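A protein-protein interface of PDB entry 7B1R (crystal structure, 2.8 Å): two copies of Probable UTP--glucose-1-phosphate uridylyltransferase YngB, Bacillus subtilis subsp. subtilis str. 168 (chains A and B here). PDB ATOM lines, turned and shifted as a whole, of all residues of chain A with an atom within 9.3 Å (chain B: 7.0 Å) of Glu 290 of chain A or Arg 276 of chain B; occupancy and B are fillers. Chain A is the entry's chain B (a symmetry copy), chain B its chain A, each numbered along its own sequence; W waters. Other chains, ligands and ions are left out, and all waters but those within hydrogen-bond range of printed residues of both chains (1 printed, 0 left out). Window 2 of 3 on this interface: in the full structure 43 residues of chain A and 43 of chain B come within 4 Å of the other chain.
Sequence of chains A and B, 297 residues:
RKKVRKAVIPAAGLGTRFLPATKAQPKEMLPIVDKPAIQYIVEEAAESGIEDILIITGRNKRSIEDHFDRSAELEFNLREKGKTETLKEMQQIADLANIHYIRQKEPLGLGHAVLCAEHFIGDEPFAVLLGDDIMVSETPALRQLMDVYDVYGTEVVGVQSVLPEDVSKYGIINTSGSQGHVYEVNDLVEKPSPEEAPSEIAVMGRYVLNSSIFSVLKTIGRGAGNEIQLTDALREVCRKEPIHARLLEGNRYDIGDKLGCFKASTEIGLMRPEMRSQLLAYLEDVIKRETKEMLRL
Met 275 of chain B touches Leu 259 of chain A (CE to CD1, 3.9 Å).
CD1 of Leu 259 of chain A touches NE2 of Gln 278 of chain B, 3.7 Å away.
Val 286 of chain A touches Leu 270 of chain B.
Ile 287 of chain A touches Glu 284 of chain B (CD1 to CA, 3.9 Å).
The guanidinium group (NH2) of Arg 276 of chain B lies within salt-bridge range of the side-chain carboxylate (OE1) of Glu 290 of chain A, 2.5 Å away.
The side-chain carboxylate of Glu 267 of chain B is in salt-bridge range of the guanidinium group of Arg 289 of chain A, 2.7 Å away.
The side-chain carboxylate of Glu 267 of chain B sits at hydrogen-bond distance from the side-chain hydroxyl of Tyr 282 of chain A, at 2.9 Å.
Water W1 lies within hydrogen-bond range of the side-chain carboxylate of Glu 284 of chain B (3.1 Å) and the side-chain hydroxyl of Thr 291 of chain A (3.5 Å).
Of the printed residues of chain B, Leu 259 of chain A touches Met 275 (3.9 Å) and Gln 278 (3.7 Å).
Of the printed residues of chain B, Arg 289 of chain A touches Glu 267.
Glu 290 of chain A touches just one residue of chain B: Arg 276 (2.5 Å).
Met 294 of chain A touches none of the printed residues of chain B.
Of chain A, only Glu 290 (2.5 Å) comes within 4 Å of Arg 276 of chain B.
No residue of chain A comes within 4 Å of Ser 277 of chain B.
Tyr 282 of chain B touches none of the printed residues of chain A.
Positions printed for both chains: 282 and 284.
OG1 of Thr 291 of chain A is in hydrogen-bond range of O of Ile 287 of chain A (3.1 Å).
O of Glu 274 of chain B sits close to OE1 of Gln 278 of chain B (2.5 Å).
NH1 of Arg 272 of chain B lies within hydrogen-bond range of SD of Met 275 of chain B (3.2 Å).
The guanidinium group of Arg 276 of chain B lies close to the backbone carbonyl oxygen of Leu 270 of chain B, at 3.2 Å.
Printed residues of chain A that touch a printed residue of chain B: Leu 259, Tyr 282, Val 286, Ile 287, Arg 289 and Glu 290.
Hydrophobic or aromatic side chains of chain A within 4 Å of the printed part of chain B: Leu 259, Tyr 282, Val 286 and Ile 287.
Of the 16 printed residues of chain B, 6 touch a printed residue of chain A.
Printed residues of chain B that touch a printed residue of chain A: Glu 267, Leu 270, Met 275, Arg 276, Gln 278 and Glu 284.
Hydrophobic or aromatic side chains of chain B that line the printed part of chain A: Leu 270 and Met 275.
Along chain B the printed residues that touch a printed residue of chain A span positions 267 to 284.
Among the printed residues, 7 pairs touch across the chains.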
ATOM      1  N   LEU A 259     -16.057  23.103  12.457  1.00  0.00           N
ATOM      2  CA  LEU A 259     -15.783  21.703  12.696  1.00  0.00           C
ATOM      3  C   LEU A 259     -16.676  21.123  13.791  1.00  0.00           C
ATOM      4  O   LEU A 259     -17.023  19.944  13.738  1.00  0.00           O
ATOM      5  CB  LEU A 259     -14.341  21.605  13.149  1.00  0.00           C
ATOM      6  CG  LEU A 259     -13.696  20.297  12.747  1.00  0.00           C
ATOM      7  CD1 LEU A 259     -12.651  20.590  11.663  1.00  0.00           C
ATOM      8  CD2 LEU A 259     -13.134  19.601  13.988  1.00  0.00           C
ATOM      9  N   TYR A 282     -19.744   5.081   4.172  1.00  0.00           N
ATOM     10  CA  TYR A 282     -19.098   6.162   3.450  1.00  0.00           C
ATOM     11  C   TYR A 282     -17.805   6.591   4.136  1.00  0.00           C
ATOM     12  O   TYR A 282     -16.858   6.932   3.423  1.00  0.00           O
ATOM     13  CB  TYR A 282     -20.003   7.379   3.286  1.00  0.00           C
ATOM     14  CG  TYR A 282     -19.260   8.588   2.780  1.00  0.00           C
ATOM     15  CD1 TYR A 282     -18.746   8.615   1.486  1.00  0.00           C
ATOM     16  CD2 TYR A 282     -19.027   9.685   3.604  1.00  0.00           C
ATOM     17  CE1 TYR A 282     -18.042   9.710   1.014  1.00  0.00           C
ATOM     18  CE2 TYR A 282     -18.315  10.785   3.153  1.00  0.00           C
ATOM     19  CZ  TYR A 282     -17.823  10.793   1.853  1.00  0.00           C
ATOM     20  OH  TYR A 282     -17.095  11.858   1.408  1.00  0.00           O
ATOM     21  N   LEU A 283     -17.751   6.587   5.488  1.00  0.00           N
ATOM     22  CA  LEU A 283     -16.541   7.087   6.138  1.00  0.00           C
ATOM     23  C   LEU A 283     -15.420   6.055   6.051  1.00  0.00           C
ATOM     24  O   LEU A 283     -14.244   6.407   5.869  1.00  0.00           O
ATOM     25  CB  LEU A 283     -16.813   7.494   7.584  1.00  0.00           C
ATOM     26  CG  LEU A 283     -17.633   8.769   7.774  1.00  0.00           C
ATOM     27  CD1 LEU A 283     -17.848   9.034   9.251  1.00  0.00           C
ATOM     28  CD2 LEU A 283     -16.988   9.976   7.081  1.00  0.00           C
ATOM     29  N   GLU A 284     -15.801   4.776   6.176  1.00  0.00           N
ATOM     30  CA  GLU A 284     -14.845   3.714   5.904  1.00  0.00           C
ATOM     31  C   GLU A 284     -14.237   3.957   4.519  1.00  0.00           C
ATOM     32  O   GLU A 284     -13.028   4.097   4.392  1.00  0.00           O
ATOM     33  CB  GLU A 284     -15.454   2.325   6.098  1.00  0.00           C
ATOM     34  CG  GLU A 284     -15.969   2.048   7.499  1.00  0.00           C
ATOM     35  CD  GLU A 284     -16.960   0.893   7.708  1.00  0.00           C
ATOM     36  OE1 GLU A 284     -17.319   0.197   6.706  1.00  0.00           O
ATOM     37  OE2 GLU A 284     -17.387   0.668   8.892  1.00  0.00           O
ATOM     38  N   ASP A 285     -15.055   4.117   3.475  1.00  0.00           N
ATOM     39  CA  ASP A 285     -14.459   4.196   2.148  1.00  0.00           C
ATOM     40  C   ASP A 285     -13.647   5.473   1.927  1.00  0.00           C
ATOM     41  O   ASP A 285     -12.666   5.424   1.191  1.00  0.00           O
ATOM     42  CB  ASP A 285     -15.253   3.533   1.012  1.00  0.00           C
ATOM     43  CG  ASP A 285     -16.770   3.694   1.054  1.00  0.00           C
ATOM     44  OD1 ASP A 285     -17.228   4.832   1.283  1.00  0.00           O
ATOM     45  OD2 ASP A 285     -17.503   2.679   0.826  1.00  0.00           O
ATOM     46  N   VAL A 286     -13.974   6.570   2.626  1.00  0.00           N
ATOM     47  CA  VAL A 286     -13.137   7.762   2.572  1.00  0.00           C
ATOM     48  C   VAL A 286     -11.763   7.497   3.194  1.00  0.00           C
ATOM     49  O   VAL A 286     -10.728   7.866   2.618  1.00  0.00           O
ATOM     50  CB  VAL A 286     -13.813   9.008   3.174  1.00  0.00           C
ATOM     51  CG1 VAL A 286     -12.819  10.136   3.461  1.00  0.00           C
ATOM     52  CG2 VAL A 286     -14.877   9.533   2.231  1.00  0.00           C
ATOM     53  N   ILE A 287     -11.749   6.869   4.377  1.00  0.00           N
ATOM     54  CA  ILE A 287     -10.471   6.531   4.982  1.00  0.00           C
ATOM     55  C   ILE A 287      -9.664   5.578   4.081  1.00  0.00           C
ATOM     56  O   ILE A 287      -8.481   5.830   3.842  1.00  0.00           O
ATOM     57  CB  ILE A 287     -10.665   6.014   6.413  1.00  0.00           C
ATOM     58  CG1 ILE A 287     -11.347   7.066   7.270  1.00  0.00           C
ATOM     59  CG2 ILE A 287      -9.341   5.601   7.033  1.00  0.00           C
ATOM     60  CD1 ILE A 287     -11.948   6.469   8.502  1.00  0.00           C
ATOM     61  N   LYS A 288     -10.279   4.498   3.554  1.00  0.00           N
ATOM     62  CA  LYS A 288      -9.541   3.677   2.594  1.00  0.00           C
ATOM     63  C   LYS A 288      -8.924   4.577   1.519  1.00  0.00           C
ATOM     64  O   LYS A 288      -7.710   4.544   1.334  1.00  0.00           O
ATOM     65  CB  LYS A 288     -10.276   2.432   2.050  1.00  0.00           C
ATOM     66  N   ARG A 289      -9.740   5.420   0.862  1.00  0.00           N
ATOM     67  CA  ARG A 289      -9.236   6.166  -0.279  1.00  0.00           C
ATOM     68  C   ARG A 289      -8.050   7.023   0.156  1.00  0.00           C
ATOM     69  O   ARG A 289      -7.107   7.197  -0.613  1.00  0.00           O
ATOM     70  CB  ARG A 289     -10.347   6.907  -1.032  1.00  0.00           C
ATOM     71  CG  ARG A 289      -9.869   7.879  -2.110  1.00  0.00           C
ATOM     72  CD  ARG A 289     -10.914   8.667  -2.916  1.00  0.00           C
ATOM     73  NE  ARG A 289     -12.039   9.197  -2.142  1.00  0.00           N
ATOM     74  CZ  ARG A 289     -11.969  10.174  -1.228  1.00  0.00           C
ATOM     75  NH1 ARG A 289     -10.820  10.776  -0.963  1.00  0.00           N
ATOM     76  NH2 ARG A 289     -13.055  10.537  -0.566  1.00  0.00           N
ATOM     77  N   GLU A 290      -8.080   7.491   1.406  1.00  0.00           N
ATOM     78  CA  GLU A 290      -7.073   8.438   1.857  1.00  0.00           C
ATOM     79  C   GLU A 290      -5.745   7.744   2.126  1.00  0.00           C
ATOM     80  O   GLU A 290      -4.698   8.340   1.918  1.00  0.00           O
ATOM     81  CB  GLU A 290      -7.570   9.250   3.050  1.00  0.00           C
ATOM     82  CG  GLU A 290      -8.576  10.325   2.653  1.00  0.00           C
ATOM     83  CD  GLU A 290      -8.287  11.217   1.442  1.00  0.00           C
ATOM     84  OE1 GLU A 290      -7.295  11.972   1.463  1.00  0.00           O
ATOM     85  OE2 GLU A 290      -9.081  11.183   0.477  1.00  0.00           O
ATOM     86  N   THR A 291      -5.806   6.488   2.577  1.00  0.00           N
ATOM     87  CA  THR A 291      -4.617   5.689   2.832  1.00  0.00           C
ATOM     88  C   THR A 291      -3.971   5.304   1.502  1.00  0.00           C
ATOM     89  O   THR A 291      -2.798   5.599   1.281  1.00  0.00           O
ATOM     90  CB  THR A 291      -4.916   4.493   3.748  1.00  0.00           C
ATOM     91  OG1 THR A 291      -5.714   4.947   4.841  1.00  0.00           O
ATOM     92  CG2 THR A 291      -3.654   3.858   4.288  1.00  0.00           C
ATOM     93  N   LYS A 292      -4.755   4.677   0.612  1.00  0.00           N
ATOM     94  CA  LYS A 292      -4.302   4.330  -0.731  1.00  0.00           C
ATOM     95  C   LYS A 292      -3.615   5.538  -1.381  1.00  0.00           C
ATOM     96  O   LYS A 292      -2.509   5.417  -1.896  1.00  0.00           O
ATOM     97  CB  LYS A 292      -5.412   3.663  -1.560  1.00  0.00           C
ATOM     98  N   GLU A 293      -4.240   6.718  -1.319  1.00  0.00           N
ATOM     99  CA  GLU A 293      -3.670   7.896  -1.962  1.00  0.00           C
ATOM    100  C   GLU A 293      -2.323   8.232  -1.326  1.00  0.00           C
ATOM    101  O   GLU A 293      -1.370   8.496  -2.060  1.00  0.00           O
ATOM    102  CB  GLU A 293      -4.635   9.088  -1.995  1.00  0.00           C
ATOM    103  N   MET A 294      -2.244   8.169   0.016  1.00  0.00           N
ATOM    104  CA  MET A 294      -1.061   8.589   0.760  1.00  0.00           C
ATOM    105  C   MET A 294       0.072   7.566   0.632  1.00  0.00           C
ATOM    106  O   MET A 294       1.201   7.852   1.021  1.00  0.00           O
ATOM    107  CB  MET A 294      -1.402   8.885   2.225  1.00  0.00           C
ATOM    108  CG  MET A 294      -1.502   7.644   3.094  1.00  0.00           C
ATOM    109  SD  MET A 294      -1.381   7.998   5.023  1.00  0.00           S
ATOM    110  CE  MET A 294      -2.355   6.696   6.137  1.00  0.00           C
ATOM    111  N   LEU A 295      -0.224   6.379   0.083  1.00  0.00           N
ATOM    112  CA  LEU A 295       0.800   5.386  -0.198  1.00  0.00           C
ATOM    113  C   LEU A 295       1.161   5.390  -1.686  1.00  0.00           C
ATOM    114  O   LEU A 295       1.190   4.336  -2.299  1.00  0.00           O
ATOM    115  CB  LEU A 295       0.267   4.011   0.215  1.00  0.00           C
ATOM    116  CG  LEU A 295       0.045   3.768   1.710  1.00  0.00           C
ATOM    117  CD1 LEU A 295      -0.121   2.274   1.998  1.00  0.00           C
ATOM    118  CD2 LEU A 295       1.175   4.359   2.551  1.00  0.00           C
ATOM    119  N   ARG A 296       1.416   6.569  -2.270  1.00  0.00           N
ATOM    120  CA  ARG A 296       1.849   6.704  -3.659  1.00  0.00           C
ATOM    121  C   ARG A 296       2.801   7.909  -3.765  1.00  0.00           C
ATOM    122  O   ARG A 296       3.397   8.272  -2.714  1.00  0.00           O
ATOM    123  CB  ARG A 296       0.666   6.744  -4.647  1.00  0.00           C
ATOM    124  N   GLU B 267     -15.950  15.797   1.090  1.00  0.00           N
ATOM    125  CA  GLU B 267     -14.992  15.798  -0.007  1.00  0.00           C
ATOM    126  C   GLU B 267     -14.291  17.153  -0.129  1.00  0.00           C
ATOM    127  O   GLU B 267     -13.055  17.206  -0.116  1.00  0.00           O
ATOM    128  CB  GLU B 267     -15.616  15.405  -1.352  1.00  0.00           C
ATOM    129  CG  GLU B 267     -16.213  14.006  -1.385  1.00  0.00           C
ATOM    130  CD  GLU B 267     -15.363  12.778  -1.087  1.00  0.00           C
ATOM    131  OE1 GLU B 267     -14.222  12.934  -0.663  1.00  0.00           O
ATOM    132  OE2 GLU B 267     -15.880  11.657  -1.264  1.00  0.00           O
ATOM    133  N   GLY B 269     -14.257  19.529   1.974  1.00  0.00           N
ATOM    134  CA  GLY B 269     -13.656  19.858   3.255  1.00  0.00           C
ATOM    135  C   GLY B 269     -12.217  19.373   3.302  1.00  0.00           C
ATOM    136  O   GLY B 269     -11.319  20.122   3.679  1.00  0.00           O
ATOM    137  N   LEU B 270     -12.038  18.121   2.870  1.00  0.00           N
ATOM    138  CA  LEU B 270     -10.749  17.452   2.808  1.00  0.00           C
ATOM    139  C   LEU B 270      -9.831  18.129   1.805  1.00  0.00           C
ATOM    140  O   LEU B 270      -8.626  17.916   1.886  1.00  0.00           O
ATOM    141  CB  LEU B 270     -10.950  15.977   2.457  1.00  0.00           C
ATOM    142  CG  LEU B 270     -11.493  15.171   3.628  1.00  0.00           C
ATOM    143  CD1 LEU B 270     -11.940  13.781   3.238  1.00  0.00           C
ATOM    144  CD2 LEU B 270     -10.460  15.126   4.738  1.00  0.00           C
ATOM    145  N   MET B 271     -10.388  18.948   0.903  1.00  0.00           N
ATOM    146  CA  MET B 271      -9.536  19.696  -0.009  1.00  0.00           C
ATOM    147  C   MET B 271      -9.103  21.029   0.616  1.00  0.00           C
ATOM    148  O   MET B 271      -8.285  21.766   0.067  1.00  0.00           O
ATOM    149  CB  MET B 271     -10.226  19.881  -1.358  1.00  0.00           C
ATOM    150  CG  MET B 271     -10.345  18.618  -2.163  1.00  0.00           C
ATOM    151  SD  MET B 271     -11.802  18.848  -3.500  1.00  0.00           S
ATOM    152  CE  MET B 271     -12.535  17.115  -4.113  1.00  0.00           C
ATOM    153  N   ARG B 272      -9.622  21.357   1.799  1.00  0.00           N
ATOM    154  CA  ARG B 272      -9.231  22.635   2.379  1.00  0.00           C
ATOM    155  C   ARG B 272      -8.138  22.397   3.408  1.00  0.00           C
ATOM    156  O   ARG B 272      -8.377  21.745   4.427  1.00  0.00           O
ATOM    157  CB  ARG B 272     -10.426  23.525   2.757  1.00  0.00           C
ATOM    158  CG  ARG B 272     -11.054  24.177   1.530  1.00  0.00           C
ATOM    159  CD  ARG B 272     -12.542  24.425   1.485  1.00  0.00           C
ATOM    160  NE  ARG B 272     -12.748  25.773   1.993  1.00  0.00           N
ATOM    161  CZ  ARG B 272     -12.984  26.083   3.265  1.00  0.00           C
ATOM    162  NH1 ARG B 272     -13.059  25.135   4.181  1.00  0.00           N
ATOM    163  NH2 ARG B 272     -13.136  27.339   3.626  1.00  0.00           N
ATOM    164  N   PRO B 273      -6.906  22.862   3.073  1.00  0.00           N
ATOM    165  CA  PRO B 273      -5.722  22.751   3.928  1.00  0.00           C
ATOM    166  C   PRO B 273      -5.915  23.090   5.401  1.00  0.00           C
ATOM    167  O   PRO B 273      -5.451  22.356   6.260  1.00  0.00           O
ATOM    168  CB  PRO B 273      -4.726  23.750   3.316  1.00  0.00           C
ATOM    169  CG  PRO B 273      -5.465  24.428   2.182  1.00  0.00           C
ATOM    170  CD  PRO B 273      -6.573  23.483   1.783  1.00  0.00           C
ATOM    171  N   GLU B 274      -6.609  24.193   5.689  1.00  0.00           N
ATOM    172  CA  GLU B 274      -6.818  24.632   7.061  1.00  0.00           C
ATOM    173  C   GLU B 274      -7.644  23.583   7.802  1.00  0.00           C
ATOM    174  O   GLU B 274      -7.527  23.442   9.016  1.00  0.00           O
ATOM    175  CB  GLU B 274      -7.457  26.028   7.114  1.00  0.00           C
ATOM    176  CG  GLU B 274      -8.789  26.168   6.364  1.00  0.00           C
ATOM    177  CD  GLU B 274      -8.853  26.114   4.828  1.00  0.00           C
ATOM    178  OE1 GLU B 274      -7.983  25.461   4.167  1.00  0.00           O
ATOM    179  OE2 GLU B 274      -9.808  26.709   4.271  1.00  0.00           O
ATOM    180  N   MET B 275      -8.458  22.835   7.050  1.00  0.00           N
ATOM    181  CA  MET B 275      -9.453  21.958   7.634  1.00  0.00           C
ATOM    182  C   MET B 275      -8.905  20.540   7.662  1.00  0.00           C
ATOM    183  O   MET B 275      -9.150  19.794   8.607  1.00  0.00           O
ATOM    184  CB  MET B 275     -10.710  21.987   6.766  1.00  0.00           C
ATOM    185  CG  MET B 275     -11.354  23.347   6.676  1.00  0.00           C
ATOM    186  SD  MET B 275     -13.299  23.171   6.690  1.00  0.00           S
ATOM    187  CE  MET B 275     -13.876  22.388   8.431  1.00  0.00           C
ATOM    188  N   ARG B 276      -8.137  20.194   6.623  1.00  0.00           N
ATOM    189  CA  ARG B 276      -7.982  18.801   6.236  1.00  0.00           C
ATOM    190  C   ARG B 276      -7.569  17.933   7.422  1.00  0.00           C
ATOM    191  O   ARG B 276      -8.165  16.885   7.675  1.00  0.00           O
ATOM    192  CB  ARG B 276      -7.048  18.642   5.035  1.00  0.00           C
ATOM    193  CG  ARG B 276      -7.108  17.245   4.437  1.00  0.00           C
ATOM    194  CD  ARG B 276      -6.022  17.114   3.396  1.00  0.00           C
ATOM    195  NE  ARG B 276      -5.622  15.719   3.327  1.00  0.00           N
ATOM    196  CZ  ARG B 276      -6.076  14.834   2.448  1.00  0.00           C
ATOM    197  NH1 ARG B 276      -6.957  15.181   1.522  1.00  0.00           N
ATOM    198  NH2 ARG B 276      -5.639  13.592   2.505  1.00  0.00           N
ATOM    199  N   SER B 277      -6.556  18.386   8.161  1.00  0.00           N
ATOM    200  CA  SER B 277      -5.958  17.524   9.164  1.00  0.00           C
ATOM    201  C   SER B 277      -6.936  17.247  10.296  1.00  0.00           C
ATOM    202  O   SER B 277      -6.999  16.108  10.731  1.00  0.00           O
ATOM    203  CB  SER B 277      -4.650  18.043   9.660  1.00  0.00           C
ATOM    204  OG  SER B 277      -4.640  19.458   9.586  1.00  0.00           O
ATOM    205  N   GLN B 278      -7.729  18.245  10.727  1.00  0.00           N
ATOM    206  CA  GLN B 278      -8.601  18.022  11.878  1.00  0.00           C
ATOM    207  C   GLN B 278      -9.756  17.098  11.486  1.00  0.00           C
ATOM    208  O   GLN B 278     -10.240  16.293  12.292  1.00  0.00           O
ATOM    209  CB  GLN B 278      -9.153  19.323  12.471  1.00  0.00           C
ATOM    210  CG  GLN B 278      -8.120  20.400  12.781  1.00  0.00           C
ATOM    211  CD  GLN B 278      -8.510  21.712  12.134  1.00  0.00           C
ATOM    212  OE1 GLN B 278      -7.904  22.146  11.155  1.00  0.00           O
ATOM    213  NE2 GLN B 278      -9.554  22.343  12.652  1.00  0.00           N
ATOM    214  N   LEU B 279     -10.175  17.241  10.227  1.00  0.00           N
ATOM    215  CA  LEU B 279     -11.335  16.570   9.679  1.00  0.00           C
ATOM    216  C   LEU B 279     -11.025  15.079   9.530  1.00  0.00           C
ATOM    217  O   LEU B 279     -11.751  14.222  10.051  1.00  0.00           O
ATOM    218  CB  LEU B 279     -11.599  17.248   8.335  1.00  0.00           C
ATOM    219  CG  LEU B 279     -12.912  16.912   7.640  1.00  0.00           C
ATOM    220  CD1 LEU B 279     -14.092  17.154   8.567  1.00  0.00           C
ATOM    221  CD2 LEU B 279     -13.043  17.746   6.372  1.00  0.00           C
ATOM    222  N   LEU B 280      -9.905  14.790   8.846  1.00  0.00           N
ATOM    223  CA  LEU B 280      -9.379  13.440   8.702  1.00  0.00           C
ATOM    224  C   LEU B 280      -9.200  12.776  10.076  1.00  0.00           C
ATOM    225  O   LEU B 280      -9.694  11.675  10.309  1.00  0.00           O
ATOM    226  CB  LEU B 280      -8.063  13.539   7.927  1.00  0.00           C
ATOM    227  CG  LEU B 280      -7.686  12.320   7.084  1.00  0.00           C
ATOM    228  CD1 LEU B 280      -8.901  11.470   6.756  1.00  0.00           C
ATOM    229  CD2 LEU B 280      -6.971  12.735   5.805  1.00  0.00           C
ATOM    230  N   ALA B 281      -8.532  13.484  10.998  1.00  0.00           N
ATOM    231  CA  ALA B 281      -8.432  13.113  12.399  1.00  0.00           C
ATOM    232  C   ALA B 281      -9.779  12.639  12.910  1.00  0.00           C
ATOM    233  O   ALA B 281      -9.899  11.492  13.317  1.00  0.00           O
ATOM    234  CB  ALA B 281      -8.001  14.295  13.225  1.00  0.00           C
ATOM    235  N   TYR B 282     -10.763  13.554  12.888  1.00  0.00           N
ATOM    236  CA  TYR B 282     -12.110  13.315  13.392  1.00  0.00           C
ATOM    237  C   TYR B 282     -12.714  12.063  12.766  1.00  0.00           C
ATOM    238  O   TYR B 282     -13.306  11.249  13.483  1.00  0.00           O
ATOM    239  CB  TYR B 282     -13.057  14.491  13.119  1.00  0.00           C
ATOM    240  CG  TYR B 282     -14.484  14.161  13.476  1.00  0.00           C
ATOM    241  CD1 TYR B 282     -14.847  13.852  14.781  1.00  0.00           C
ATOM    242  CD2 TYR B 282     -15.461  14.093  12.497  1.00  0.00           C
ATOM    243  CE1 TYR B 282     -16.145  13.489  15.108  1.00  0.00           C
ATOM    244  CE2 TYR B 282     -16.757  13.701  12.801  1.00  0.00           C
ATOM    245  CZ  TYR B 282     -17.106  13.403  14.114  1.00  0.00           C
ATOM    246  OH  TYR B 282     -18.392  13.040  14.441  1.00  0.00           O
ATOM    247  N   GLU B 284     -11.262   9.317  11.160  1.00  0.00           N
ATOM    248  CA  GLU B 284     -10.575   8.144  11.696  1.00  0.00           C
ATOM    249  C   GLU B 284     -11.087   7.831  13.106  1.00  0.00           C
ATOM    250  O   GLU B 284     -11.424   6.688  13.413  1.00  0.00           O
ATOM    251  CB  GLU B 284      -9.051   8.316  11.671  1.00  0.00           C
ATOM    252  CG  GLU B 284      -8.417   7.950  10.333  1.00  0.00           C
ATOM    253  CD  GLU B 284      -7.059   8.563   9.990  1.00  0.00           C
ATOM    254  OE1 GLU B 284      -6.522   9.312  10.832  1.00  0.00           O
ATOM    255  OE2 GLU B 284      -6.533   8.302   8.865  1.00  0.00           O
HETATM  256  O   HOH W   1      -5.417   8.209   6.009  1.00  0.00           O
